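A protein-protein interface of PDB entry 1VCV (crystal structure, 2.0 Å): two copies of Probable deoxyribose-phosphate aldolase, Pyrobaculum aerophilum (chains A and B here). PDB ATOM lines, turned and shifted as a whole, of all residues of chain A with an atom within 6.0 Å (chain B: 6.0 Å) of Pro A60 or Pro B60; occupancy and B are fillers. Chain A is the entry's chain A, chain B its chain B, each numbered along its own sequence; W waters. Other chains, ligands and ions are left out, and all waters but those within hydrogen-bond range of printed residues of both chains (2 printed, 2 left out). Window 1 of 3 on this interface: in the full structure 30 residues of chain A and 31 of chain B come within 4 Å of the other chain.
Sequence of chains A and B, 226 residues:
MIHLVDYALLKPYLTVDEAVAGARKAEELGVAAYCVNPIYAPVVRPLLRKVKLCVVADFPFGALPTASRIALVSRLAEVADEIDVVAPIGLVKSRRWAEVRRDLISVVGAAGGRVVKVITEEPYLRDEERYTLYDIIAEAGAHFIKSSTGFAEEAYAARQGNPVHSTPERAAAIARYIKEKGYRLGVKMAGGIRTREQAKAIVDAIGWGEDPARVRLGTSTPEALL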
ATOM      1  N   PRO A  12     -11.237   7.342  -2.948  1.00  0.00           N
ATOM      2  CA  PRO A  12      -9.781   7.319  -3.138  1.00  0.00           C
ATOM      3  C   PRO A  12      -9.328   7.151  -4.591  1.00  0.00           C
ATOM      4  O   PRO A  12      -8.205   7.528  -4.951  1.00  0.00           O
ATOM      5  CB  PRO A  12      -9.334   6.164  -2.238  1.00  0.00           C
ATOM      6  CG  PRO A  12     -10.505   5.220  -2.293  1.00  0.00           C
ATOM      7  CD  PRO A  12     -11.698   6.161  -2.190  1.00  0.00           C
ATOM      8  N   ASP A  58      -7.661  13.127   8.365  1.00  0.00           N
ATOM      9  CA  ASP A  58      -7.610  11.841   9.062  1.00  0.00           C
ATOM     10  C   ASP A  58      -8.915  11.127   8.742  1.00  0.00           C
ATOM     11  O   ASP A  58      -9.596  10.592   9.618  1.00  0.00           O
ATOM     12  CB  ASP A  58      -7.462  12.055  10.568  1.00  0.00           C
ATOM     13  CG  ASP A  58      -7.057  10.787  11.295  1.00  0.00           C
ATOM     14  OD1 ASP A  58      -6.714   9.793  10.622  1.00  0.00           O
ATOM     15  OD2 ASP A  58      -7.073  10.781  12.541  1.00  0.00           O
ATOM     16  N   PHE A  59      -9.222  11.129   7.448  1.00  0.00           N
ATOM     17  CA  PHE A  59     -10.441  10.586   6.879  1.00  0.00           C
ATOM     18  C   PHE A  59     -10.211   9.271   6.123  1.00  0.00           C
ATOM     19  O   PHE A  59      -9.225   9.124   5.397  1.00  0.00           O
ATOM     20  CB  PHE A  59     -11.000  11.673   5.956  1.00  0.00           C
ATOM     21  CG  PHE A  59     -12.333  11.364   5.362  1.00  0.00           C
ATOM     22  CD1 PHE A  59     -12.434  10.644   4.169  1.00  0.00           C
ATOM     23  CD2 PHE A  59     -13.495  11.826   5.971  1.00  0.00           C
ATOM     24  CE1 PHE A  59     -13.675  10.396   3.593  1.00  0.00           C
ATOM     25  CE2 PHE A  59     -14.741  11.578   5.401  1.00  0.00           C
ATOM     26  CZ  PHE A  59     -14.831  10.864   4.210  1.00  0.00           C
ATOM     27  N   PRO A  60     -11.147   8.311   6.250  1.00  0.00           N
ATOM     28  CA  PRO A  60     -12.379   8.392   7.039  1.00  0.00           C
ATOM     29  C   PRO A  60     -12.377   7.719   8.415  1.00  0.00           C
ATOM     30  O   PRO A  60     -13.416   7.686   9.074  1.00  0.00           O
ATOM     31  CB  PRO A  60     -13.395   7.746   6.116  1.00  0.00           C
ATOM     32  CG  PRO A  60     -12.606   6.589   5.581  1.00  0.00           C
ATOM     33  CD  PRO A  60     -11.231   7.195   5.285  1.00  0.00           C
ATOM     34  N   PHE A  61     -11.231   7.203   8.852  1.00  0.00           N
ATOM     35  CA  PHE A  61     -11.134   6.503  10.140  1.00  0.00           C
ATOM     36  C   PHE A  61     -10.965   7.336  11.408  1.00  0.00           C
ATOM     37  O   PHE A  61     -11.452   6.946  12.475  1.00  0.00           O
ATOM     38  CB  PHE A  61      -9.990   5.489  10.108  1.00  0.00           C
ATOM     39  CG  PHE A  61     -10.260   4.273   9.268  1.00  0.00           C
ATOM     40  CD1 PHE A  61     -11.415   4.167   8.499  1.00  0.00           C
ATOM     41  CD2 PHE A  61      -9.342   3.226   9.248  1.00  0.00           C
ATOM     42  CE1 PHE A  61     -11.654   3.037   7.724  1.00  0.00           C
ATOM     43  CE2 PHE A  61      -9.570   2.085   8.471  1.00  0.00           C
ATOM     44  CZ  PHE A  61     -10.726   1.991   7.710  1.00  0.00           C
ATOM     45  N   GLY A  62     -10.262   8.458  11.303  1.00  0.00           N
ATOM     46  CA  GLY A  62     -10.031   9.288  12.471  1.00  0.00           C
ATOM     47  C   GLY A  62      -9.187   8.506  13.457  1.00  0.00           C
ATOM     48  O   GLY A  62      -9.288   8.692  14.675  1.00  0.00           O
ATOM     49  N   VAL A  86     -12.447  13.901  11.100  1.00  0.00           N
ATOM     50  CA  VAL A  86     -13.141  12.798  11.760  1.00  0.00           C
ATOM     51  C   VAL A  86     -12.814  12.770  13.253  1.00  0.00           C
ATOM     52  O   VAL A  86     -11.663  12.975  13.654  1.00  0.00           O
ATOM     53  CB  VAL A  86     -12.726  11.436  11.141  1.00  0.00           C
ATOM     54  CG1 VAL A  86     -13.572  10.305  11.734  1.00  0.00           C
ATOM     55  CG2 VAL A  86     -12.874  11.488   9.620  1.00  0.00           C
ATOM     56  N   ILE A  89     -13.005   8.227  16.528  1.00  0.00           N
ATOM     57  CA  ILE A  89     -14.019   7.184  16.666  1.00  0.00           C
ATOM     58  C   ILE A  89     -13.673   6.072  17.642  1.00  0.00           C
ATOM     59  O   ILE A  89     -14.475   5.734  18.521  1.00  0.00           O
ATOM     60  CB  ILE A  89     -14.366   6.549  15.298  1.00  0.00           C
ATOM     61  CG1 ILE A  89     -14.855   7.635  14.330  1.00  0.00           C
ATOM     62  CG2 ILE A  89     -15.454   5.490  15.482  1.00  0.00           C
ATOM     63  CD1 ILE A  89     -15.331   7.105  12.979  1.00  0.00           C
ATOM     64  N   GLU A 121     -19.651  10.620  12.840  1.00  0.00           N
ATOM     65  CA  GLU A 121     -19.943   9.281  12.318  1.00  0.00           C
ATOM     66  C   GLU A 121     -21.104   8.670  13.098  1.00  0.00           C
ATOM     67  O   GLU A 121     -20.978   7.611  13.724  1.00  0.00           O
ATOM     68  CB  GLU A 121     -18.706   8.374  12.386  1.00  0.00           C
ATOM     69  CG  GLU A 121     -18.791   7.127  11.490  1.00  0.00           C
ATOM     70  CD  GLU A 121     -18.763   7.457   9.996  1.00  0.00           C
ATOM     71  OE1 GLU A 121     -19.680   8.153   9.511  1.00  0.00           O
ATOM     72  OE2 GLU A 121     -17.816   7.021   9.308  1.00  0.00           O
ATOM     73  N   THR A 149     -19.050  10.219   7.565  1.00  0.00           N
ATOM     74  CA  THR A 149     -18.008  10.205   6.551  1.00  0.00           C
ATOM     75  C   THR A 149     -18.516   9.768   5.178  1.00  0.00           C
ATOM     76  O   THR A 149     -17.973  10.179   4.153  1.00  0.00           O
ATOM     77  CB  THR A 149     -16.854   9.250   6.952  1.00  0.00           C
ATOM     78  OG1 THR A 149     -17.329   7.899   6.954  1.00  0.00           O
ATOM     79  CG2 THR A 149     -16.327   9.593   8.350  1.00  0.00           C
ATOM     80  N   PHE A 151     -18.654   6.589   4.548  1.00  0.00           N
ATOM     81  CA  PHE A 151     -17.996   5.303   4.396  1.00  0.00           C
ATOM     82  C   PHE A 151     -18.256   4.365   5.573  1.00  0.00           C
ATOM     83  O   PHE A 151     -17.522   3.398   5.775  1.00  0.00           O
ATOM     84  CB  PHE A 151     -16.490   5.508   4.208  1.00  0.00           C
ATOM     85  CG  PHE A 151     -16.138   6.252   2.948  1.00  0.00           C
ATOM     86  CD1 PHE A 151     -16.200   7.640   2.902  1.00  0.00           C
ATOM     87  CD2 PHE A 151     -15.780   5.557   1.793  1.00  0.00           C
ATOM     88  CE1 PHE A 151     -15.913   8.331   1.726  1.00  0.00           C
ATOM     89  CE2 PHE A 151     -15.493   6.237   0.616  1.00  0.00           C
ATOM     90  CZ  PHE A 151     -15.558   7.629   0.581  1.00  0.00           C
ATOM     91  N   PRO B  12     -12.047   1.186  12.279  1.00  0.00           N
ATOM     92  CA  PRO B  12     -11.957   2.443  13.034  1.00  0.00           C
ATOM     93  C   PRO B  12     -12.686   2.418  14.375  1.00  0.00           C
ATOM     94  O   PRO B  12     -12.340   3.162  15.292  1.00  0.00           O
ATOM     95  CB  PRO B  12     -12.538   3.475  12.065  1.00  0.00           C
ATOM     96  CG  PRO B  12     -13.507   2.670  11.245  1.00  0.00           C
ATOM     97  CD  PRO B  12     -12.737   1.392  10.991  1.00  0.00           C
ATOM     98  N   ASP B  58      -1.718   6.683   6.392  1.00  0.00           N
ATOM     99  CA  ASP B  58      -2.566   7.346   5.402  1.00  0.00           C
ATOM    100  C   ASP B  58      -3.467   6.253   4.852  1.00  0.00           C
ATOM    101  O   ASP B  58      -3.601   6.065   3.642  1.00  0.00           O
ATOM    102  CB  ASP B  58      -1.715   7.965   4.292  1.00  0.00           C
ATOM    103  CG  ASP B  58      -2.530   8.837   3.363  1.00  0.00           C
ATOM    104  OD1 ASP B  58      -3.649   9.235   3.761  1.00  0.00           O
ATOM    105  OD2 ASP B  58      -2.053   9.132   2.250  1.00  0.00           O
ATOM    106  N   PHE B  59      -4.102   5.561   5.794  1.00  0.00           N
ATOM    107  CA  PHE B  59      -4.955   4.407   5.544  1.00  0.00           C
ATOM    108  C   PHE B  59      -6.439   4.706   5.796  1.00  0.00           C
ATOM    109  O   PHE B  59      -6.794   5.351   6.784  1.00  0.00           O
ATOM    110  CB  PHE B  59      -4.443   3.295   6.463  1.00  0.00           C
ATOM    111  CG  PHE B  59      -5.082   1.959   6.245  1.00  0.00           C
ATOM    112  CD1 PHE B  59      -6.218   1.590   6.960  1.00  0.00           C
ATOM    113  CD2 PHE B  59      -4.523   1.049   5.356  1.00  0.00           C
ATOM    114  CE1 PHE B  59      -6.782   0.338   6.797  1.00  0.00           C
ATOM    115  CE2 PHE B  59      -5.080  -0.212   5.182  1.00  0.00           C
ATOM    116  CZ  PHE B  59      -6.211  -0.570   5.904  1.00  0.00           C
ATOM    117  N   PRO B  60      -7.330   4.190   4.933  1.00  0.00           N
ATOM    118  CA  PRO B  60      -7.039   3.354   3.763  1.00  0.00           C
ATOM    119  C   PRO B  60      -7.072   4.029   2.383  1.00  0.00           C
ATOM    120  O   PRO B  60      -6.983   3.336   1.368  1.00  0.00           O
ATOM    121  CB  PRO B  60      -8.103   2.275   3.871  1.00  0.00           C
ATOM    122  CG  PRO B  60      -9.304   3.096   4.266  1.00  0.00           C
ATOM    123  CD  PRO B  60      -8.752   4.068   5.311  1.00  0.00           C
ATOM    124  N   PHE B  61      -7.187   5.356   2.338  1.00  0.00           N
ATOM    125  CA  PHE B  61      -7.256   6.080   1.059  1.00  0.00           C
ATOM    126  C   PHE B  61      -5.932   6.415   0.360  1.00  0.00           C
ATOM    127  O   PHE B  61      -5.859   6.416  -0.875  1.00  0.00           O
ATOM    128  CB  PHE B  61      -8.033   7.390   1.236  1.00  0.00           C
ATOM    129  CG  PHE B  61      -9.522   7.218   1.365  1.00  0.00           C
ATOM    130  CD1 PHE B  61     -10.092   5.960   1.544  1.00  0.00           C
ATOM    131  CD2 PHE B  61     -10.358   8.338   1.341  1.00  0.00           C
ATOM    132  CE1 PHE B  61     -11.477   5.812   1.699  1.00  0.00           C
ATOM    133  CE2 PHE B  61     -11.742   8.208   1.495  1.00  0.00           C
ATOM    134  CZ  PHE B  61     -12.302   6.937   1.676  1.00  0.00           C
ATOM    135  N   GLY B  62      -4.901   6.727   1.141  1.00  0.00           N
ATOM    136  CA  GLY B  62      -3.620   7.095   0.563  1.00  0.00           C
ATOM    137  C   GLY B  62      -3.762   8.414  -0.178  1.00  0.00           C
ATOM    138  O   GLY B  62      -3.011   8.699  -1.120  1.00  0.00           O
ATOM    139  N   VAL B  86      -0.351   3.294   2.308  1.00  0.00           N
ATOM    140  CA  VAL B  86      -1.154   3.161   1.095  1.00  0.00           C
ATOM    141  C   VAL B  86      -0.556   3.987  -0.038  1.00  0.00           C
ATOM    142  O   VAL B  86      -0.143   5.134   0.163  1.00  0.00           O
ATOM    143  CB  VAL B  86      -2.622   3.634   1.319  1.00  0.00           C
ATOM    144  CG1 VAL B  86      -3.453   3.394   0.053  1.00  0.00           C
ATOM    145  CG2 VAL B  86      -3.230   2.907   2.506  1.00  0.00           C
ATOM    146  N   ILE B  89      -3.340   6.068  -4.525  1.00  0.00           N
ATOM    147  CA  ILE B  89      -4.344   5.501  -5.422  1.00  0.00           C
ATOM    148  C   ILE B  89      -4.917   6.441  -6.483  1.00  0.00           C
ATOM    149  O   ILE B  89      -4.970   6.091  -7.662  1.00  0.00           O
ATOM    150  CB  ILE B  89      -5.508   4.899  -4.611  1.00  0.00           C
ATOM    151  CG1 ILE B  89      -4.960   3.870  -3.616  1.00  0.00           C
ATOM    152  CG2 ILE B  89      -6.509   4.237  -5.552  1.00  0.00           C
ATOM    153  CD1 ILE B  89      -6.003   3.291  -2.687  1.00  0.00           C
ATOM    154  N   GLU B 121      -3.571  -1.936  -3.375  1.00  0.00           N
ATOM    155  CA  GLU B 121      -5.027  -1.964  -3.532  1.00  0.00           C
ATOM    156  C   GLU B 121      -5.355  -2.549  -4.901  1.00  0.00           C
ATOM    157  O   GLU B 121      -5.982  -1.907  -5.750  1.00  0.00           O
ATOM    158  CB  GLU B 121      -5.644  -0.566  -3.397  1.00  0.00           C
ATOM    159  CG  GLU B 121      -7.156  -0.599  -3.106  1.00  0.00           C
ATOM    160  CD  GLU B 121      -7.484  -1.229  -1.748  1.00  0.00           C
ATOM    161  OE1 GLU B 121      -7.131  -2.408  -1.528  1.00  0.00           O
ATOM    162  OE2 GLU B 121      -8.096  -0.546  -0.896  1.00  0.00           O
ATOM    163  N   THR B 149      -5.968  -3.023   1.120  1.00  0.00           N
ATOM    164  CA  THR B 149      -6.206  -2.429   2.437  1.00  0.00           C
ATOM    165  C   THR B 149      -7.156  -3.268   3.277  1.00  0.00           C
ATOM    166  O   THR B 149      -7.080  -3.266   4.507  1.00  0.00           O
ATOM    167  CB  THR B 149      -6.848  -1.026   2.332  1.00  0.00           C
ATOM    168  OG1 THR B 149      -8.166  -1.151   1.780  1.00  0.00           O
ATOM    169  CG2 THR B 149      -6.012  -0.104   1.460  1.00  0.00           C
ATOM    170  N   PHE B 151     -10.323  -2.788   2.749  1.00  0.00           N
ATOM    171  CA  PHE B 151     -11.493  -1.915   2.729  1.00  0.00           C
ATOM    172  C   PHE B 151     -11.868  -1.477   1.310  1.00  0.00           C
ATOM    173  O   PHE B 151     -12.566  -0.477   1.115  1.00  0.00           O
ATOM    174  CB  PHE B 151     -11.250  -0.678   3.606  1.00  0.00           C
ATOM    175  CG  PHE B 151     -11.028  -0.998   5.064  1.00  0.00           C
ATOM    176  CD1 PHE B 151      -9.769  -1.373   5.526  1.00  0.00           C
ATOM    177  CD2 PHE B 151     -12.089  -0.952   5.968  1.00  0.00           C
ATOM    178  CE1 PHE B 151      -9.566  -1.702   6.868  1.00  0.00           C
ATOM    179  CE2 PHE B 151     -11.901  -1.279   7.316  1.00  0.00           C
ATOM    180  CZ  PHE B 151     -10.636  -1.656   7.769  1.00  0.00           C
HETATM  181  O   HOH W   1      -8.455   7.280   7.754  1.00  0.00           O
HETATM  182  O   HOH W   2      -7.355   7.529   4.468  1.00  0.00           O
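The side-chain hydroxyl of Thr B149 sits at hydrogen-bond distance from the backbone NH of Phe B151 (2.9 Å). OG1 of Thr A149 is in hydrogen-bond range of N of Phe A151.
Among the printed residues, pairs that only touch across the chains: Phe A151 with Phe B61, Phe A61 with Phe B151, Phe A59 with Phe B61, Phe A61 with Pro B12, Phe A61 with Phe B59, Phe A61 with Pro B60, Pro A12 with Phe B61, Pro A12 with Ile B89, Pro A60 with Phe B61, Ile A89 with Pro B12 and Pro A60 with Pro B60.
Printed residues of chain B within 4 Å of Phe A61: Pro B12, Phe B59, Pro B60 and Phe B151. Of the printed residues of chain A, Pro B12 touches Phe A61 (3.7 Å) and Ile A89 (3.9 Å). Printed residues of chain A within 4 Å of Ile B89: Pro A12. The nearest printed residue of chain A that does not touch Pro B60 is Phe A59 (5.1 Å). The nearest printed residue of chain A that does not touch Pro B12 is Pro A60 (5.2 Å).
Of the 11 printed residues of chain A, 6 touch a printed residue of chain B. Hydrophobic or aromatic side chains of chain A that line the printed part of chain B: Pro A12, Phe A59, Pro A60, Phe A61, Ile A89 and Phe A151. Along chain A the printed residues that touch a printed residue of chain B span positions 12 to 151. Printed residues of chain B that touch a printed residue of chain A: Pro B12, Phe B59, Pro B60, Phe B61, Ile B89 and Phe B151. Hydrophobic or aromatic side chains of chain B that line the printed part of chain A: Pro B12, Phe B59, Pro B60, Phe B61, Ile B89 and Phe B151.
Pro A12 touches Phe B61, and with the chains exchanged Phe A61 touches Pro B12. Pro A12 touches Ile B89, and with the chains exchanged Ile A89 touches Pro B12. Phe A59 touches Phe B61, and with the chains exchanged Phe A61 touches Phe B59. Phe A61 touches Phe B151, and with the chains exchanged Phe A151 touches Phe B61. Of the 11 pairs that touch across the chains among the printed residues, 11 have their exchanged pair printed and touching as well.
Water W2 lies within hydrogen-bond range of the backbone carbonyl oxygen of Phe A59 (2.6 Å), the backbone NH of Phe B61 (3.0 Å) and the backbone carbonyl oxygen of Phe B59 (3.2 Å). Water W1 lies within hydrogen-bond range of the backbone carbonyl oxygen of Phe B59 (2.7 Å), the backbone NH of Phe A61 (3.0 Å) and the backbone carbonyl oxygen of Phe A59 (3.1 Å).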
